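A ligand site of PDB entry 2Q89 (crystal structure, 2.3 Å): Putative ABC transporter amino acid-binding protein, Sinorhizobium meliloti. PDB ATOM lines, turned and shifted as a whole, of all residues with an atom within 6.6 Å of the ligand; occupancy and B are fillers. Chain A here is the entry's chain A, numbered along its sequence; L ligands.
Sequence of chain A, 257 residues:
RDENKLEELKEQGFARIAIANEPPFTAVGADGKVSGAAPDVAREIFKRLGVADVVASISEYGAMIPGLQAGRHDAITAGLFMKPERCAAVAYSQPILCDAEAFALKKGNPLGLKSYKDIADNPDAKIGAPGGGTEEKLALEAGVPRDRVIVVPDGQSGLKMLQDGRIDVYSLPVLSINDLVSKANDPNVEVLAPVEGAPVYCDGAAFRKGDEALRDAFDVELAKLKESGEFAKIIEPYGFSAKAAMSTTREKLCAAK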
ATOM      1  N   GLU A  22      -8.469  15.218  19.864  1.00  0.00           N
ATOM      2  CA  GLU A  22      -7.980  16.387  19.123  1.00  0.00           C
ATOM      3  C   GLU A  22      -9.125  16.969  18.284  1.00  0.00           C
ATOM      4  O   GLU A  22      -9.356  16.542  17.155  1.00  0.00           O
ATOM      5  CB  GLU A  22      -6.818  15.964  18.216  1.00  0.00           C
ATOM      6  CG  GLU A  22      -6.211  17.074  17.370  1.00  0.00           C
ATOM      7  CD  GLU A  22      -5.250  16.551  16.316  1.00  0.00           C
ATOM      8  OE1 GLU A  22      -4.331  15.776  16.654  1.00  0.00           O
ATOM      9  OE2 GLU A  22      -5.418  16.926  15.136  1.00  0.00           O
ATOM     10  N   PHE A  25     -11.488  16.533  15.172  1.00  0.00           N
ATOM     11  CA  PHE A  25     -11.404  15.147  14.744  1.00  0.00           C
ATOM     12  C   PHE A  25     -12.030  14.238  15.807  1.00  0.00           C
ATOM     13  O   PHE A  25     -12.917  13.426  15.513  1.00  0.00           O
ATOM     14  CB  PHE A  25      -9.948  14.727  14.465  1.00  0.00           C
ATOM     15  CG  PHE A  25      -9.388  15.323  13.197  1.00  0.00           C
ATOM     16  CD1 PHE A  25      -8.809  16.587  13.196  1.00  0.00           C
ATOM     17  CD2 PHE A  25      -9.452  14.625  12.006  1.00  0.00           C
ATOM     18  CE1 PHE A  25      -8.294  17.138  12.034  1.00  0.00           C
ATOM     19  CE2 PHE A  25      -8.935  15.164  10.833  1.00  0.00           C
ATOM     20  CZ  PHE A  25      -8.356  16.421  10.847  1.00  0.00           C
ATOM     21  N   TYR A  61      -1.011   9.047  18.759  1.00  0.00           N
ATOM     22  CA  TYR A  61      -1.190   8.544  17.398  1.00  0.00           C
ATOM     23  C   TYR A  61      -0.289   7.363  17.041  1.00  0.00           C
ATOM     24  O   TYR A  61      -0.684   6.490  16.277  1.00  0.00           O
ATOM     25  CB  TYR A  61      -1.024   9.679  16.373  1.00  0.00           C
ATOM     26  CG  TYR A  61      -2.182  10.655  16.380  1.00  0.00           C
ATOM     27  CD1 TYR A  61      -3.360  10.376  15.680  1.00  0.00           C
ATOM     28  CD2 TYR A  61      -2.095  11.849  17.093  1.00  0.00           C
ATOM     29  CE1 TYR A  61      -4.433  11.263  15.701  1.00  0.00           C
ATOM     30  CE2 TYR A  61      -3.170  12.745  17.112  1.00  0.00           C
ATOM     31  CZ  TYR A  61      -4.324  12.448  16.411  1.00  0.00           C
ATOM     32  OH  TYR A  61      -5.381  13.324  16.421  1.00  0.00           O
ATOM     33  N   ALA A  78      -9.940   8.296  14.339  1.00  0.00           N
ATOM     34  CA  ALA A  78      -9.239   9.347  15.071  1.00  0.00           C
ATOM     35  C   ALA A  78      -8.640  10.436  14.185  1.00  0.00           C
ATOM     36  O   ALA A  78      -7.937  11.319  14.676  1.00  0.00           O
ATOM     37  CB  ALA A  78      -8.161   8.712  15.943  1.00  0.00           C
ATOM     38  N   GLY A  79      -8.904  10.369  12.883  1.00  0.00           N
ATOM     39  CA  GLY A  79      -8.243  11.230  11.913  1.00  0.00           C
ATOM     40  C   GLY A  79      -6.887  10.686  11.504  1.00  0.00           C
ATOM     41  O   GLY A  79      -6.017  11.436  11.068  1.00  0.00           O
ATOM     42  N   LEU A  80      -6.708   9.364  11.633  1.00  0.00           N
ATOM     43  CA  LEU A  80      -5.442   8.724  11.262  1.00  0.00           C
ATOM     44  C   LEU A  80      -5.288   8.674   9.742  1.00  0.00           C
ATOM     45  O   LEU A  80      -5.808   7.772   9.065  1.00  0.00           O
ATOM     46  CB  LEU A  80      -5.326   7.319  11.888  1.00  0.00           C
ATOM     47  CG  LEU A  80      -3.939   6.667  11.810  1.00  0.00           C
ATOM     48  CD1 LEU A  80      -2.987   7.255  12.863  1.00  0.00           C
ATOM     49  CD2 LEU A  80      -4.038   5.166  11.989  1.00  0.00           C
ATOM     50  N   PHE A  81      -4.562   9.665   9.225  1.00  0.00           N
ATOM     51  CA  PHE A  81      -4.456   9.885   7.789  1.00  0.00           C
ATOM     52  C   PHE A  81      -3.852   8.701   7.035  1.00  0.00           C
ATOM     53  O   PHE A  81      -2.932   8.042   7.524  1.00  0.00           O
ATOM     54  CB  PHE A  81      -3.666  11.151   7.490  1.00  0.00           C
ATOM     55  CG  PHE A  81      -4.332  12.414   7.987  1.00  0.00           C
ATOM     56  CD1 PHE A  81      -5.697  12.619   7.805  1.00  0.00           C
ATOM     57  CD2 PHE A  81      -3.578  13.407   8.614  1.00  0.00           C
ATOM     58  CE1 PHE A  81      -6.308  13.784   8.249  1.00  0.00           C
ATOM     59  CE2 PHE A  81      -4.185  14.585   9.063  1.00  0.00           C
ATOM     60  CZ  PHE A  81      -5.546  14.770   8.885  1.00  0.00           C
ATOM     61  N   MET A  82      -4.396   8.436   5.845  1.00  0.00           N
ATOM     62  CA  MET A  82      -3.933   7.336   4.993  1.00  0.00           C
ATOM     63  C   MET A  82      -2.582   7.648   4.397  1.00  0.00           C
ATOM     64  O   MET A  82      -2.378   8.699   3.758  1.00  0.00           O
ATOM     65  CB  MET A  82      -4.938   7.047   3.871  1.00  0.00           C
ATOM     66  CG  MET A  82      -6.287   6.551   4.338  1.00  0.00           C
ATOM     67  SD  MET A  82      -7.280   5.929   2.968  1.00  0.00           S
ATOM     68  CE  MET A  82      -8.929   6.278   3.552  1.00  0.00           C
ATOM     69  N   LYS A  83      -1.639   6.735   4.614  1.00  0.00           N
ATOM     70  CA  LYS A  83      -0.293   6.811   4.074  1.00  0.00           C
ATOM     71  C   LYS A  83       0.075   5.421   3.599  1.00  0.00           C
ATOM     72  O   LYS A  83      -0.339   4.434   4.231  1.00  0.00           O
ATOM     73  CB  LYS A  83       0.693   7.246   5.163  1.00  0.00           C
ATOM     74  CG  LYS A  83       0.638   8.700   5.558  1.00  0.00           C
ATOM     75  CD  LYS A  83       1.187   8.904   6.981  1.00  0.00           C
ATOM     76  CE  LYS A  83       2.686   8.721   7.043  1.00  0.00           C
ATOM     77  NZ  LYS A  83       3.217   8.816   8.449  1.00  0.00           N
ATOM     78  N   ARG A  86       1.115   3.094   6.353  1.00  0.00           N
ATOM     79  CA  ARG A  86      -0.032   2.799   7.230  1.00  0.00           C
ATOM     80  C   ARG A  86      -1.010   1.854   6.531  1.00  0.00           C
ATOM     81  O   ARG A  86      -1.533   0.932   7.152  1.00  0.00           O
ATOM     82  CB  ARG A  86      -0.759   4.085   7.635  1.00  0.00           C
ATOM     83  CG  ARG A  86       0.005   4.962   8.614  1.00  0.00           C
ATOM     84  CD  ARG A  86      -0.793   6.176   9.063  1.00  0.00           C
ATOM     85  NE  ARG A  86      -0.074   6.967  10.055  1.00  0.00           N
ATOM     86  CZ  ARG A  86      -0.433   8.188  10.457  1.00  0.00           C
ATOM     87  NH1 ARG A  86      -1.503   8.777   9.930  1.00  0.00           N
ATOM     88  NH2 ARG A  86       0.287   8.825  11.365  1.00  0.00           N
ATOM     89  N   TYR A  92      -7.999  -0.023   5.691  1.00  0.00           N
ATOM     90  CA  TYR A  92      -8.683   1.248   5.770  1.00  0.00           C
ATOM     91  C   TYR A  92     -10.062   1.189   5.110  1.00  0.00           C
ATOM     92  O   TYR A  92     -10.273   0.424   4.170  1.00  0.00           O
ATOM     93  CB  TYR A  92      -7.857   2.339   5.083  1.00  0.00           C
ATOM     94  CG  TYR A  92      -6.937   3.119   6.005  1.00  0.00           C
ATOM     95  CD1 TYR A  92      -7.456   3.921   7.029  1.00  0.00           C
ATOM     96  CD2 TYR A  92      -5.555   3.086   5.834  1.00  0.00           C
ATOM     97  CE1 TYR A  92      -6.615   4.643   7.875  1.00  0.00           C
ATOM     98  CE2 TYR A  92      -4.706   3.808   6.673  1.00  0.00           C
ATOM     99  CZ  TYR A  92      -5.243   4.586   7.693  1.00  0.00           C
ATOM    100  OH  TYR A  92      -4.413   5.303   8.524  1.00  0.00           O
ATOM    101  N   GLU A 101      -2.253  20.682   6.600  1.00  0.00           N
ATOM    102  CA  GLU A 101      -1.438  20.852   7.811  1.00  0.00           C
ATOM    103  C   GLU A 101      -1.247  22.325   8.143  1.00  0.00           C
ATOM    104  O   GLU A 101      -1.178  23.176   7.240  1.00  0.00           O
ATOM    105  CB  GLU A 101      -0.056  20.191   7.648  1.00  0.00           C
ATOM    106  CG  GLU A 101      -0.060  18.683   7.373  1.00  0.00           C
ATOM    107  CD  GLU A 101      -0.332  17.860   8.611  1.00  0.00           C
ATOM    108  OE1 GLU A 101      -0.914  18.385   9.592  1.00  0.00           O
ATOM    109  OE2 GLU A 101       0.032  16.661   8.626  1.00  0.00           O
ATOM    110  N   ALA A 129       5.003  18.329  17.764  1.00  0.00           N
ATOM    111  CA  ALA A 129       4.182  17.466  16.921  1.00  0.00           C
ATOM    112  C   ALA A 129       3.738  16.247  17.735  1.00  0.00           C
ATOM    113  O   ALA A 129       4.436  15.857  18.680  1.00  0.00           O
ATOM    114  CB  ALA A 129       4.979  17.027  15.693  1.00  0.00           C
ATOM    115  N   PRO A 130       2.589  15.662  17.408  1.00  0.00           N
ATOM    116  CA  PRO A 130       2.160  14.393  18.038  1.00  0.00           C
ATOM    117  C   PRO A 130       3.112  13.253  17.693  1.00  0.00           C
ATOM    118  O   PRO A 130       3.651  13.230  16.582  1.00  0.00           O
ATOM    119  CB  PRO A 130       0.788  14.126  17.416  1.00  0.00           C
ATOM    120  CG  PRO A 130       0.360  15.402  16.811  1.00  0.00           C
ATOM    121  CD  PRO A 130       1.592  16.151  16.438  1.00  0.00           C
ATOM    122  N   GLY A 131       3.337  12.334  18.630  1.00  0.00           N
ATOM    123  CA  GLY A 131       4.223  11.189  18.394  1.00  0.00           C
ATOM    124  C   GLY A 131       3.604  10.183  17.444  1.00  0.00           C
ATOM    125  O   GLY A 131       2.462   9.763  17.621  1.00  0.00           O
ATOM    126  N   GLY A 132       4.373   9.826  16.414  1.00  0.00           N
ATOM    127  CA  GLY A 132       3.934   8.850  15.398  1.00  0.00           C
ATOM    128  C   GLY A 132       3.017   9.432  14.330  1.00  0.00           C
ATOM    129  O   GLY A 132       2.554   8.698  13.442  1.00  0.00           O
ATOM    130  N   GLY A 133       2.746  10.725  14.407  1.00  0.00           N
ATOM    131  CA  GLY A 133       1.813  11.380  13.490  1.00  0.00           C
ATOM    132  C   GLY A 133       2.429  11.896  12.202  1.00  0.00           C
ATOM    133  O   GLY A 133       3.637  11.757  11.982  1.00  0.00           O
ATOM    134  N   THR A 134       1.599  12.496  11.351  1.00  0.00           N
ATOM    135  CA  THR A 134       2.025  12.923  10.009  1.00  0.00           C
ATOM    136  C   THR A 134       3.020  14.081  10.032  1.00  0.00           C
ATOM    137  O   THR A 134       3.980  14.076   9.262  1.00  0.00           O
ATOM    138  CB  THR A 134       0.821  13.274   9.095  1.00  0.00           C
ATOM    139  OG1 THR A 134      -0.101  14.109   9.812  1.00  0.00           O
ATOM    140  CG2 THR A 134       0.016  12.022   8.771  1.00  0.00           C
ATOM    141  N   GLU A 135       2.781  15.053  10.914  1.00  0.00           N
ATOM    142  CA  GLU A 135       3.595  16.276  11.013  1.00  0.00           C
ATOM    143  C   GLU A 135       5.015  15.983  11.460  1.00  0.00           C
ATOM    144  O   GLU A 135       5.964  16.583  10.955  1.00  0.00           O
ATOM    145  CB  GLU A 135       2.963  17.281  11.996  1.00  0.00           C
ATOM    146  CG  GLU A 135       1.531  17.675  11.687  1.00  0.00           C
ATOM    147  CD  GLU A 135       0.509  16.738  12.298  1.00  0.00           C
ATOM    148  OE1 GLU A 135       0.865  15.928  13.183  1.00  0.00           O
ATOM    149  OE2 GLU A 135      -0.672  16.802  11.889  1.00  0.00           O
ATOM    150  N   GLU A 136       5.156  15.083  12.434  1.00  0.00           N
ATOM    151  CA  GLU A 136       6.447  14.624  12.908  1.00  0.00           C
ATOM    152  C   GLU A 136       7.255  14.020  11.766  1.00  0.00           C
ATOM    153  O   GLU A 136       8.410  14.380  11.545  1.00  0.00           O
ATOM    154  CB  GLU A 136       6.276  13.579  14.015  1.00  0.00           C
ATOM    155  CG  GLU A 136       7.559  12.820  14.354  1.00  0.00           C
ATOM    156  CD  GLU A 136       7.372  11.799  15.440  1.00  0.00           C
ATOM    157  OE1 GLU A 136       7.934  12.002  16.529  1.00  0.00           O
ATOM    158  OE2 GLU A 136       6.650  10.797  15.218  1.00  0.00           O
ATOM    159  N   SER A 171       2.541  21.928  15.340  1.00  0.00           N
ATOM    160  CA  SER A 171       1.932  21.573  14.059  1.00  0.00           C
ATOM    161  C   SER A 171       0.867  20.476  14.167  1.00  0.00           C
ATOM    162  O   SER A 171       1.157  19.360  14.593  1.00  0.00           O
ATOM    163  CB  SER A 171       3.020  21.179  13.043  1.00  0.00           C
ATOM    164  OG  SER A 171       2.479  21.003  11.740  1.00  0.00           O
ATOM    165  N   LEU A 172      -0.355  20.813  13.756  1.00  0.00           N
ATOM    166  CA  LEU A 172      -1.457  19.857  13.634  1.00  0.00           C
ATOM    167  C   LEU A 172      -2.173  20.139  12.310  1.00  0.00           C
ATOM    168  O   LEU A 172      -1.753  21.043  11.580  1.00  0.00           O
ATOM    169  CB  LEU A 172      -2.436  20.003  14.816  1.00  0.00           C
ATOM    170  CG  LEU A 172      -2.024  19.623  16.250  1.00  0.00           C
ATOM    171  CD1 LEU A 172      -3.152  19.914  17.239  1.00  0.00           C
ATOM    172  CD2 LEU A 172      -1.605  18.168  16.332  1.00  0.00           C
ATOM    173  N   PRO A 173      -3.231  19.389  11.976  1.00  0.00           N
ATOM    174  CA  PRO A 173      -4.086  19.771  10.856  1.00  0.00           C
ATOM    175  C   PRO A 173      -4.751  21.128  11.079  1.00  0.00           C
ATOM    176  O   PRO A 173      -4.989  21.517  12.221  1.00  0.00           O
ATOM    177  CB  PRO A 173      -5.160  18.663  10.827  1.00  0.00           C
ATOM    178  CG  PRO A 173      -4.553  17.519  11.549  1.00  0.00           C
ATOM    179  CD  PRO A 173      -3.676  18.128  12.604  1.00  0.00           C
ATOM    180  N   SER A 176      -7.741  21.423  13.507  1.00  0.00           N
ATOM    181  CA  SER A 176      -7.277  21.213  14.882  1.00  0.00           C
ATOM    182  C   SER A 176      -6.585  22.463  15.448  1.00  0.00           C
ATOM    183  O   SER A 176      -6.882  22.880  16.563  1.00  0.00           O
ATOM    184  CB  SER A 176      -6.311  20.033  14.954  1.00  0.00           C
ATOM    185  OG  SER A 176      -6.864  18.855  14.396  1.00  0.00           O
ATOM    186  N   ASP A 203      -8.224  10.694   6.170  1.00  0.00           N
ATOM    187  CA  ASP A 203      -8.211   9.491   6.974  1.00  0.00           C
ATOM    188  C   ASP A 203      -9.313   8.516   6.537  1.00  0.00           C
ATOM    189  O   ASP A 203     -10.075   8.796   5.601  1.00  0.00           O
ATOM    190  CB  ASP A 203      -8.391   9.840   8.458  1.00  0.00           C
ATOM    191  CG  ASP A 203      -9.866   9.927   8.877  1.00  0.00           C
ATOM    192  OD1 ASP A 203     -10.743  10.168   8.022  1.00  0.00           O
ATOM    193  OD2 ASP A 203     -10.244   9.748  10.056  1.00  0.00           O
HETATM  194  O1  LIG L   1      -0.892  11.224  12.112  1.00  0.00           O
HETATM  195  C1  LIG L   1      -2.042  11.597  11.817  1.00  0.00           C
HETATM  196  O2  LIG L   1      -2.869  10.902  11.179  1.00  0.00           O
HETATM  197  C2  LIG L   1      -2.477  13.022  12.256  1.00  0.00           C
HETATM  198  N1  LIG L   1      -3.950  13.130  12.263  1.00  0.00           N
HETATM  199  C3  LIG L   1      -4.605  14.030  13.113  1.00  0.00           C
HETATM  200  C4  LIG L   1      -6.123  14.124  13.082  1.00  0.00           C
HETATM  201  N2  LIG L   1      -3.904  14.840  14.019  1.00  0.00           N
HETATM  202  C5  LIG L   1      -2.439  14.797  14.077  1.00  0.00           C
HETATM  203  C6  LIG L   1      -1.883  13.436  13.625  1.00  0.00           C
HETATM  204  O3  LIG L   1      -0.479  13.606  13.515  1.00  0.00           O
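NH2 of Arg 86 is in salt-bridge range of O1 of the ligand, 2.8 Å away. The backbone carbonyl oxygen (O) of Gly 79 sits close to a nitrogen (N1) of the ligand (2.9 Å). OE2 of Glu 22 is in hydrogen-bond range of N2 of the ligand, at 2.8 Å. The side-chain carboxylate (OE1) of Glu 135 sits at hydrogen-bond distance from an oxygen (O3) of the ligand, at 2.7 Å. N of Phe 81 lies within hydrogen-bond range of O2 of the ligand, at 2.9 Å. A nitrogen (N2) of the ligand lies within hydrogen-bond range of the side-chain hydroxyl (OH) of Tyr 61, 3.2 Å away. The backbone NH (N) of Thr 134 lies within hydrogen-bond range of an oxygen (O1) of the ligand (2.9 Å).
OE2 of Glu 22 lies within hydrogen-bond range of OG of Ser 176, at 2.5 Å. The side-chain carboxylate of Glu 135 is in hydrogen-bond range of the side-chain hydroxyl of Thr 134 (3.4 Å). OE2 of Glu 101 sits at hydrogen-bond distance from OG1 of Thr 134, 2.8 Å away. The guanidinium group (NH2) of Arg 86 lies within hydrogen-bond range of the backbone carbonyl oxygen (O) of Gly 132 (3.1 Å). The backbone carbonyl oxygen (O) of Phe 81 is in hydrogen-bond range of the guanidinium group (NH1) of Arg 86, 2.9 Å away. The backbone carbonyl oxygen (O) of Leu 80 is in hydrogen-bond range of the side-chain hydroxyl (OH) of Tyr 92 (2.9 Å). The side-chain hydroxyl (OH) of Tyr 92 lies within hydrogen-bond range of the backbone carbonyl oxygen (O) of Phe 81 (3.3 Å). The backbone NH (N) of Gly 79 sits close to the side-chain carboxylate (OD2) of Asp 203 (3.2 Å).
Residues that only touch the ligand: Gly 133, Leu 80, Phe 25, Pro 173, Ala 78 and Pro 130. Hydrophobic or aromatic side chains that line the ligand: Phe 25, Tyr 61, Phe 81, Pro 130 and Pro 173. 13 residues have an atom within 4 Å of the ligand: Glu 22, Phe 25, Tyr 61, Ala 78, Gly 79, Leu 80, Phe 81, Arg 86, Pro 130, Gly 133, Thr 134, Glu 135 and Pro 173.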
